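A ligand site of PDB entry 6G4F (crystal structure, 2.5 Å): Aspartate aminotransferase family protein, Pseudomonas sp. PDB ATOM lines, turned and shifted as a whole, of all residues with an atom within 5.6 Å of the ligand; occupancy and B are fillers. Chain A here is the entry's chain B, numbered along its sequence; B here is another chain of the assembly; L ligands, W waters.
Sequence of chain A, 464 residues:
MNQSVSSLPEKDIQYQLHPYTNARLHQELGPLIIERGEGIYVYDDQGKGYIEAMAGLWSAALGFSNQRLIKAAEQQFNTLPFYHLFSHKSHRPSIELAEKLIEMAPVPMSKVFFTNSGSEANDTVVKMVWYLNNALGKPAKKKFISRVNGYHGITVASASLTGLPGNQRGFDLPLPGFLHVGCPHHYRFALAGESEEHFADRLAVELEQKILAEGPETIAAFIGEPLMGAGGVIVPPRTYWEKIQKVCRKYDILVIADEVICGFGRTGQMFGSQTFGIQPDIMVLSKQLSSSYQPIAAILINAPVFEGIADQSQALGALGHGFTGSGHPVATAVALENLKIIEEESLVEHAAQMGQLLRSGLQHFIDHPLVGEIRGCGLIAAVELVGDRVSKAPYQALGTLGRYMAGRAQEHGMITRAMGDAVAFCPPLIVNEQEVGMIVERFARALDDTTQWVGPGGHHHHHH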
ATOM      1  N   TRP A  58     -25.007  14.293  -2.916  1.00  0.00           N
ATOM      2  CA  TRP A  58     -25.091  15.544  -3.632  1.00  0.00           C
ATOM      3  C   TRP A  58     -24.848  15.364  -5.126  1.00  0.00           C
ATOM      4  O   TRP A  58     -24.473  16.313  -5.802  1.00  0.00           O
ATOM      5  CB  TRP A  58     -24.055  16.530  -3.103  1.00  0.00           C
ATOM      6  CG  TRP A  58     -23.787  16.545  -1.611  1.00  0.00           C
ATOM      7  CD1 TRP A  58     -22.926  15.731  -0.923  1.00  0.00           C
ATOM      8  CD2 TRP A  58     -24.305  17.468  -0.658  1.00  0.00           C
ATOM      9  NE1 TRP A  58     -22.913  16.060   0.405  1.00  0.00           N
ATOM     10  CE2 TRP A  58     -23.740  17.141   0.594  1.00  0.00           C
ATOM     11  CE3 TRP A  58     -25.192  18.551  -0.736  1.00  0.00           C
ATOM     12  CZ2 TRP A  58     -24.049  17.852   1.771  1.00  0.00           C
ATOM     13  CZ3 TRP A  58     -25.494  19.247   0.433  1.00  0.00           C
ATOM     14  CH2 TRP A  58     -24.936  18.886   1.676  1.00  0.00           C
ATOM     15  N   ASN A 116     -10.193  10.207 -10.792  1.00  0.00           N
ATOM     16  CA  ASN A 116     -11.334   9.408 -10.364  1.00  0.00           C
ATOM     17  C   ASN A 116     -12.185  10.178  -9.380  1.00  0.00           C
ATOM     18  O   ASN A 116     -13.401  10.139  -9.480  1.00  0.00           O
ATOM     19  CB  ASN A 116     -10.892   8.093  -9.732  1.00  0.00           C
ATOM     20  CG  ASN A 116      -9.976   7.298 -10.634  1.00  0.00           C
ATOM     21  OD1 ASN A 116     -10.406   6.755 -11.652  1.00  0.00           O
ATOM     22  ND2 ASN A 116      -8.711   7.228 -10.274  1.00  0.00           N
ATOM     23  N   SER A 117     -11.560  10.870  -8.432  1.00  0.00           N
ATOM     24  CA  SER A 117     -12.312  11.517  -7.362  1.00  0.00           C
ATOM     25  C   SER A 117     -12.022  12.998  -7.215  1.00  0.00           C
ATOM     26  O   SER A 117     -11.039  13.511  -7.738  1.00  0.00           O
ATOM     27  CB  SER A 117     -12.018  10.852  -6.029  1.00  0.00           C
ATOM     28  OG  SER A 117     -10.658  10.992  -5.731  1.00  0.00           O
ATOM     29  N   GLY A 118     -12.911  13.671  -6.502  1.00  0.00           N
ATOM     30  CA  GLY A 118     -12.718  15.060  -6.139  1.00  0.00           C
ATOM     31  C   GLY A 118     -11.492  15.192  -5.273  1.00  0.00           C
ATOM     32  O   GLY A 118     -10.708  16.123  -5.449  1.00  0.00           O
ATOM     33  N   SER A 119     -11.310  14.272  -4.329  1.00  0.00           N
ATOM     34  CA  SER A 119     -10.157  14.328  -3.437  1.00  0.00           C
ATOM     35  C   SER A 119      -8.873  14.211  -4.225  1.00  0.00           C
ATOM     36  O   SER A 119      -7.958  14.978  -4.041  1.00  0.00           O
ATOM     37  CB  SER A 119     -10.243  13.228  -2.390  1.00  0.00           C
ATOM     38  OG  SER A 119     -11.400  13.376  -1.613  1.00  0.00           O
ATOM     39  N   GLU A 120      -8.815  13.273  -5.147  1.00  0.00           N
ATOM     40  CA  GLU A 120      -7.691  13.185  -6.045  1.00  0.00           C
ATOM     41  C   GLU A 120      -7.518  14.454  -6.874  1.00  0.00           C
ATOM     42  O   GLU A 120      -6.398  14.859  -7.183  1.00  0.00           O
ATOM     43  CB  GLU A 120      -7.896  12.040  -7.037  1.00  0.00           C
ATOM     44  CG  GLU A 120      -7.611  10.635  -6.551  1.00  0.00           C
ATOM     45  CD  GLU A 120      -8.024   9.609  -7.599  1.00  0.00           C
ATOM     46  OE1 GLU A 120      -8.781   9.988  -8.538  1.00  0.00           O
ATOM     47  OE2 GLU A 120      -7.608   8.419  -7.513  1.00  0.00           O
ATOM     48  N   ASN A 122      -8.372  17.682  -6.207  1.00  0.00           N
ATOM     49  CA  ASN A 122      -7.789  18.777  -5.412  1.00  0.00           C
ATOM     50  C   ASN A 122      -6.364  18.477  -4.963  1.00  0.00           C
ATOM     51  O   ASN A 122      -5.517  19.359  -4.943  1.00  0.00           O
ATOM     52  CB  ASN A 122      -8.678  19.116  -4.209  1.00  0.00           C
ATOM     53  CG  ASN A 122      -9.952  19.857  -4.612  1.00  0.00           C
ATOM     54  OD1 ASN A 122      -9.927  20.703  -5.493  1.00  0.00           O
ATOM     55  ND2 ASN A 122     -11.053  19.594  -3.915  1.00  0.00           N
ATOM     56  N   TYR A 151     -15.148  21.877   2.594  1.00  0.00           N
ATOM     57  CA  TYR A 151     -14.785  20.489   2.359  1.00  0.00           C
ATOM     58  C   TYR A 151     -14.200  20.332   0.959  1.00  0.00           C
ATOM     59  O   TYR A 151     -14.800  20.788   0.001  1.00  0.00           O
ATOM     60  CB  TYR A 151     -16.014  19.585   2.538  1.00  0.00           C
ATOM     61  CG  TYR A 151     -15.663  18.107   2.440  1.00  0.00           C
ATOM     62  CD1 TYR A 151     -15.153  17.428   3.517  1.00  0.00           C
ATOM     63  CD2 TYR A 151     -15.844  17.412   1.247  1.00  0.00           C
ATOM     64  CE1 TYR A 151     -14.841  16.064   3.421  1.00  0.00           C
ATOM     65  CE2 TYR A 151     -15.532  16.055   1.139  1.00  0.00           C
ATOM     66  CZ  TYR A 151     -15.039  15.392   2.224  1.00  0.00           C
ATOM     67  OH  TYR A 151     -14.715  14.051   2.108  1.00  0.00           O
ATOM     68  N   HIS A 152     -13.030  19.708   0.852  1.00  0.00           N
ATOM     69  CA  HIS A 152     -12.364  19.549  -0.455  1.00  0.00           C
ATOM     70  C   HIS A 152     -11.771  18.153  -0.641  1.00  0.00           C
ATOM     71  O   HIS A 152     -10.899  17.949  -1.491  1.00  0.00           O
ATOM     72  CB  HIS A 152     -11.229  20.584  -0.607  1.00  0.00           C
ATOM     73  CG  HIS A 152     -11.701  22.005  -0.481  1.00  0.00           C
ATOM     74  ND1 HIS A 152     -12.443  22.639  -1.450  1.00  0.00           N
ATOM     75  CD2 HIS A 152     -11.542  22.905   0.523  1.00  0.00           C
ATOM     76  CE1 HIS A 152     -12.728  23.859  -1.047  1.00  0.00           C
ATOM     77  NE2 HIS A 152     -12.194  24.049   0.141  1.00  0.00           N
ATOM     78  N   GLY A 153     -12.239  17.191   0.140  1.00  0.00           N
ATOM     79  CA  GLY A 153     -11.736  15.835  -0.002  1.00  0.00           C
ATOM     80  C   GLY A 153     -10.913  15.399   1.178  1.00  0.00           C
ATOM     81  O   GLY A 153     -10.715  16.163   2.112  1.00  0.00           O
ATOM     82  N   ILE A 154     -10.388  14.178   1.096  1.00  0.00           N
ATOM     83  CA  ILE A 154      -9.820  13.540   2.256  1.00  0.00           C
ATOM     84  C   ILE A 154      -8.543  12.763   2.000  1.00  0.00           C
ATOM     85  O   ILE A 154      -8.188  11.876   2.776  1.00  0.00           O
ATOM     86  CB  ILE A 154     -10.854  12.653   2.971  1.00  0.00           C
ATOM     87  CG1 ILE A 154     -11.725  11.879   1.984  1.00  0.00           C
ATOM     88  CG2 ILE A 154     -11.762  13.505   3.853  1.00  0.00           C
ATOM     89  CD1 ILE A 154     -10.993  10.741   1.309  1.00  0.00           C
ATOM     90  N   GLU A 225     -15.309  26.402  -2.325  1.00  0.00           N
ATOM     91  CA  GLU A 225     -16.581  26.037  -2.927  1.00  0.00           C
ATOM     92  C   GLU A 225     -17.362  27.337  -3.072  1.00  0.00           C
ATOM     93  O   GLU A 225     -17.392  28.144  -2.144  1.00  0.00           O
ATOM     94  CB  GLU A 225     -17.365  25.075  -2.039  1.00  0.00           C
ATOM     95  CG  GLU A 225     -16.617  23.842  -1.560  1.00  0.00           C
ATOM     96  CD  GLU A 225     -17.254  23.242  -0.334  1.00  0.00           C
ATOM     97  OE1 GLU A 225     -18.292  22.566  -0.494  1.00  0.00           O
ATOM     98  OE2 GLU A 225     -16.753  23.463   0.775  1.00  0.00           O
ATOM     99  N   ALA A 230     -20.913  20.281   2.214  1.00  0.00           N
ATOM    100  CA  ALA A 230     -20.884  19.395   3.376  1.00  0.00           C
ATOM    101  C   ALA A 230     -20.786  20.123   4.689  1.00  0.00           C
ATOM    102  O   ALA A 230     -21.205  19.592   5.718  1.00  0.00           O
ATOM    103  CB  ALA A 230     -19.726  18.410   3.238  1.00  0.00           C
ATOM    104  N   ASP A 258     -13.867  25.094  -6.237  1.00  0.00           N
ATOM    105  CA  ASP A 258     -14.227  23.703  -6.060  1.00  0.00           C
ATOM    106  C   ASP A 258     -15.702  23.556  -6.368  1.00  0.00           C
ATOM    107  O   ASP A 258     -16.535  23.865  -5.538  1.00  0.00           O
ATOM    108  CB  ASP A 258     -13.930  23.216  -4.647  1.00  0.00           C
ATOM    109  CG  ASP A 258     -14.156  21.735  -4.486  1.00  0.00           C
ATOM    110  OD1 ASP A 258     -14.962  21.188  -5.280  1.00  0.00           O
ATOM    111  OD2 ASP A 258     -13.552  21.104  -3.568  1.00  0.00           O
ATOM    112  N   VAL A 260     -17.236  20.686  -7.220  1.00  0.00           N
ATOM    113  CA  VAL A 260     -17.616  19.284  -7.112  1.00  0.00           C
ATOM    114  C   VAL A 260     -19.119  19.133  -6.829  1.00  0.00           C
ATOM    115  O   VAL A 260     -19.778  18.280  -7.422  1.00  0.00           O
ATOM    116  CB  VAL A 260     -16.729  18.565  -6.076  1.00  0.00           C
ATOM    117  CG1 VAL A 260     -17.377  17.294  -5.559  1.00  0.00           C
ATOM    118  CG2 VAL A 260     -15.379  18.257  -6.675  1.00  0.00           C
ATOM    119  N   ILE A 261     -19.683  19.983  -5.983  1.00  0.00           N
ATOM    120  CA  ILE A 261     -21.133  19.923  -5.749  1.00  0.00           C
ATOM    121  C   ILE A 261     -21.914  20.894  -6.628  1.00  0.00           C
ATOM    122  O   ILE A 261     -22.933  20.525  -7.251  1.00  0.00           O
ATOM    123  CB  ILE A 261     -21.468  20.166  -4.270  1.00  0.00           C
ATOM    124  CG1 ILE A 261     -21.138  18.920  -3.460  1.00  0.00           C
ATOM    125  CG2 ILE A 261     -22.943  20.542  -4.086  1.00  0.00           C
ATOM    126  CD1 ILE A 261     -21.344  19.073  -1.963  1.00  0.00           C
ATOM    127  N   SER A 286     -16.874  17.116 -10.300  1.00  0.00           N
ATOM    128  CA  SER A 286     -17.167  15.702 -10.127  1.00  0.00           C
ATOM    129  C   SER A 286     -18.669  15.546  -9.917  1.00  0.00           C
ATOM    130  O   SER A 286     -19.439  16.358 -10.418  1.00  0.00           O
ATOM    131  CB  SER A 286     -16.390  15.128  -8.938  1.00  0.00           C
ATOM    132  OG  SER A 286     -16.264  13.731  -9.087  1.00  0.00           O
ATOM    133  N   LYS A 287     -19.061  14.485  -9.203  1.00  0.00           N
ATOM    134  CA  LYS A 287     -20.454  14.305  -8.706  1.00  0.00           C
ATOM    135  C   LYS A 287     -21.449  14.396  -9.905  1.00  0.00           C
ATOM    136  O   LYS A 287     -21.557  13.436 -10.718  1.00  0.00           O
ATOM    137  CB  LYS A 287     -20.723  15.139  -7.374  1.00  0.00           C
ATOM    138  CG  LYS A 287     -19.940  14.754  -6.097  1.00  0.00           C
ATOM    139  CD  LYS A 287     -20.159  15.440  -4.705  1.00  0.00           C
ATOM    140  CE  LYS A 287     -19.572  14.651  -3.479  1.00  0.00           C
ATOM    141  NZ  LYS A 287     -18.991  15.415  -2.311  1.00  0.00           N
ATOM    142  N   PHE B  86     -21.471   5.550   3.275  1.00  0.00           N
ATOM    143  CA  PHE B  86     -21.355   6.470   4.408  1.00  0.00           C
ATOM    144  C   PHE B  86     -22.494   6.223   5.383  1.00  0.00           C
ATOM    145  O   PHE B  86     -23.557   5.714   4.983  1.00  0.00           O
ATOM    146  CB  PHE B  86     -21.478   7.944   3.979  1.00  0.00           C
ATOM    147  CG  PHE B  86     -20.358   8.462   3.101  1.00  0.00           C
ATOM    148  CD1 PHE B  86     -19.477   7.621   2.422  1.00  0.00           C
ATOM    149  CD2 PHE B  86     -20.228   9.846   2.892  1.00  0.00           C
ATOM    150  CE1 PHE B  86     -18.485   8.136   1.600  1.00  0.00           C
ATOM    151  CE2 PHE B  86     -19.246  10.362   2.070  1.00  0.00           C
ATOM    152  CZ  PHE B  86     -18.375   9.510   1.418  1.00  0.00           C
ATOM    153  N   ASN B 116     -11.170   4.368  -4.984  1.00  0.00           N
ATOM    154  CA  ASN B 116     -11.162   4.333  -6.442  1.00  0.00           C
ATOM    155  C   ASN B 116      -9.803   3.921  -6.967  1.00  0.00           C
ATOM    156  O   ASN B 116      -9.727   3.138  -7.899  1.00  0.00           O
ATOM    157  CB  ASN B 116     -11.551   5.686  -7.031  1.00  0.00           C
ATOM    158  CG  ASN B 116     -12.864   6.215  -6.487  1.00  0.00           C
ATOM    159  OD1 ASN B 116     -13.941   5.674  -6.769  1.00  0.00           O
ATOM    160  ND2 ASN B 116     -12.790   7.271  -5.689  1.00  0.00           N
ATOM    161  N   GLU B 120      -5.089   6.609  -3.960  1.00  0.00           N
ATOM    162  CA  GLU B 120      -5.993   6.873  -2.859  1.00  0.00           C
ATOM    163  C   GLU B 120      -5.861   5.812  -1.755  1.00  0.00           C
ATOM    164  O   GLU B 120      -5.991   6.122  -0.577  1.00  0.00           O
ATOM    165  CB  GLU B 120      -7.435   6.834  -3.334  1.00  0.00           C
ATOM    166  CG  GLU B 120      -7.973   8.069  -4.052  1.00  0.00           C
ATOM    167  CD  GLU B 120      -9.366   7.807  -4.625  1.00  0.00           C
ATOM    168  OE1 GLU B 120      -9.755   6.622  -4.701  1.00  0.00           O
ATOM    169  OE2 GLU B 120     -10.060   8.780  -4.998  1.00  0.00           O
ATOM    170  N   GLY B 322     -13.414   8.934   3.692  1.00  0.00           N
ATOM    171  CA  GLY B 322     -14.245   8.253   2.712  1.00  0.00           C
ATOM    172  C   GLY B 322     -14.383   9.023   1.415  1.00  0.00           C
ATOM    173  O   GLY B 322     -14.539  10.234   1.416  1.00  0.00           O
ATOM    174  N   PHE B 323     -14.326   8.289   0.310  1.00  0.00           N
ATOM    175  CA  PHE B 323     -14.526   8.849  -1.005  1.00  0.00           C
ATOM    176  C   PHE B 323     -15.964   8.604  -1.458  1.00  0.00           C
ATOM    177  O   PHE B 323     -16.567   7.576  -1.143  1.00  0.00           O
ATOM    178  CB  PHE B 323     -13.569   8.197  -1.970  1.00  0.00           C
ATOM    179  CG  PHE B 323     -12.137   8.330  -1.565  1.00  0.00           C
ATOM    180  CD1 PHE B 323     -11.417   9.448  -1.907  1.00  0.00           C
ATOM    181  CD2 PHE B 323     -11.495   7.323  -0.853  1.00  0.00           C
ATOM    182  CE1 PHE B 323     -10.089   9.556  -1.562  1.00  0.00           C
ATOM    183  CE2 PHE B 323     -10.165   7.427  -0.485  1.00  0.00           C
ATOM    184  CZ  PHE B 323      -9.458   8.548  -0.857  1.00  0.00           C
ATOM    185  N   THR B 324     -16.496   9.564  -2.195  1.00  0.00           N
ATOM    186  CA  THR B 324     -17.813   9.442  -2.794  1.00  0.00           C
ATOM    187  C   THR B 324     -17.986   8.103  -3.527  1.00  0.00           C
ATOM    188  O   THR B 324     -19.011   7.418  -3.367  1.00  0.00           O
ATOM    189  CB  THR B 324     -18.055  10.632  -3.728  1.00  0.00           C
ATOM    190  OG1 THR B 324     -18.151  11.820  -2.933  1.00  0.00           O
ATOM    191  CG2 THR B 324     -19.349  10.475  -4.511  1.00  0.00           C
ATOM    192  N   GLY B 325     -16.956   7.700  -4.265  1.00  0.00           N
ATOM    193  CA  GLY B 325     -16.968   6.446  -4.990  1.00  0.00           C
ATOM    194  C   GLY B 325     -16.506   5.210  -4.216  1.00  0.00           C
ATOM    195  O   GLY B 325     -16.388   4.138  -4.819  1.00  0.00           O
HETATM  196  N1  LIG L   1     -14.981  18.547  -2.879  1.00  0.00           N
HETATM  197  C1  LIG L   1     -16.237  18.816  -2.475  1.00  0.00           C
HETATM  198  C2  LIG L   1     -16.767  20.227  -2.495  1.00  0.00           C
HETATM  199  C3  LIG L   1     -17.131  17.742  -2.021  1.00  0.00           C
HETATM  200  O1  LIG L   1     -18.376  18.031  -1.647  1.00  0.00           O
HETATM  201  C4  LIG L   1     -16.661  16.351  -2.029  1.00  0.00           C
HETATM  202  C5  LIG L   1     -17.653  15.254  -1.594  1.00  0.00           C
HETATM  203  C6  LIG L   1     -15.233  16.222  -2.508  1.00  0.00           C
HETATM  204  C7  LIG L   1     -14.478  17.318  -2.870  1.00  0.00           C
HETATM  205  C8  LIG L   1     -14.473  14.937  -2.578  1.00  0.00           C
HETATM  206  O2  LIG L   1     -14.784  14.180  -3.729  1.00  0.00           O
HETATM  207  P1  LIG L   1     -14.536  12.612  -3.578  1.00  0.00           P
HETATM  208  O3  LIG L   1     -14.917  12.053  -4.962  1.00  0.00           O
HETATM  209  O4  LIG L   1     -15.462  12.175  -2.472  1.00  0.00           O
HETATM  210  O5  LIG L   1     -13.073  12.504  -3.208  1.00  0.00           O
HETATM  211  O   HOH W   1     -16.924  12.302  -6.710  1.00  0.00           O
HETATM  212  O   HOH W   2     -14.911   9.264  -5.539  1.00  0.00           O
HETATM  213  O   HOH W   3     -15.861  12.554   0.240  1.00  0.00           O
HETATM  214  O   HOH W   4     -18.948  19.878   0.285  1.00  0.00           O
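The side-chain amino group of Lys 287 is bonded to a carbon (C5) of the ligand. The backbone NH (N) of Ser 119 sits at hydrogen-bond distance from an oxygen (O5) of the ligand. OG of Ser 119 is in hydrogen-bond range of O5 of the ligand, 2.5 Å away. The backbone NH of Thr 324 of chain B lies within hydrogen-bond range of an oxygen (O4) of the ligand (2.8 Å). An oxygen (O4) of the ligand is in hydrogen-bond range of the side-chain hydroxyl (OG1) of Thr 324 of chain B. O3 of the ligand is in hydrogen-bond range of N of Gly 118, 3.0 Å away.
The backbone NH (N) of Ile 154 is in hydrogen-bond range of the side-chain hydroxyl (OG) of Ser 119, 3.0 Å away. OD1 of Asp 258 lies within hydrogen-bond range of N of Val 260 (3.0 Å). The side-chain carboxylate (OD2) of Asp 258 lies within hydrogen-bond range of a ring nitrogen (ND1) of His 152 (2.8 Å). The side-chain carboxylate (OD2) of Asp 258 sits at hydrogen-bond distance from the side-chain amide nitrogen (ND2) of Asn 122. The side-chain carboxylate (OE2) of Glu 225 sits at hydrogen-bond distance from the backbone NH (N) of Tyr 151 (2.9 Å). N of Ser 117 is in hydrogen-bond range of OE1 of Glu 120 of chain A (2.9 Å). The side-chain hydroxyl (OG) of Ser 117 lies within hydrogen-bond range of the side-chain carboxylate (OE2) of Glu 120 of chain B (2.4 Å). The side-chain amide nitrogen of Asn 122 is in hydrogen-bond range of the backbone carbonyl oxygen of His 152.
The side-chain carboxylate (OD2) of Asp 258 sits close to a nitrogen (N1) of the ligand (3.0 Å). Residues that only touch the ligand: Ser 117, Tyr 151, His 152, Gly 153, Glu 225, Val 260, Ile 261 and Phe 323 of chain B.
Water W1 bridges O3 of the ligand and OG of Ser 286. Water W4 lies within hydrogen-bond range of O1 of the ligand (2.7 Å), N of Ala 230 (2.8 Å) and OE1 of Glu 225 (2.9 Å). Water W3 lies within hydrogen-bond range of the side-chain hydroxyl of Tyr 151, an oxygen (O4) of the ligand and the backbone carbonyl oxygen of Gly 322 of chain B. Water W2 lies within hydrogen-bond range of an oxygen (O3) of the ligand (2.8 Å), the backbone NH of Gly 325 of chain B (2.9 Å) and the side-chain amide nitrogen of Asn 116 of chain B (2.9 Å).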
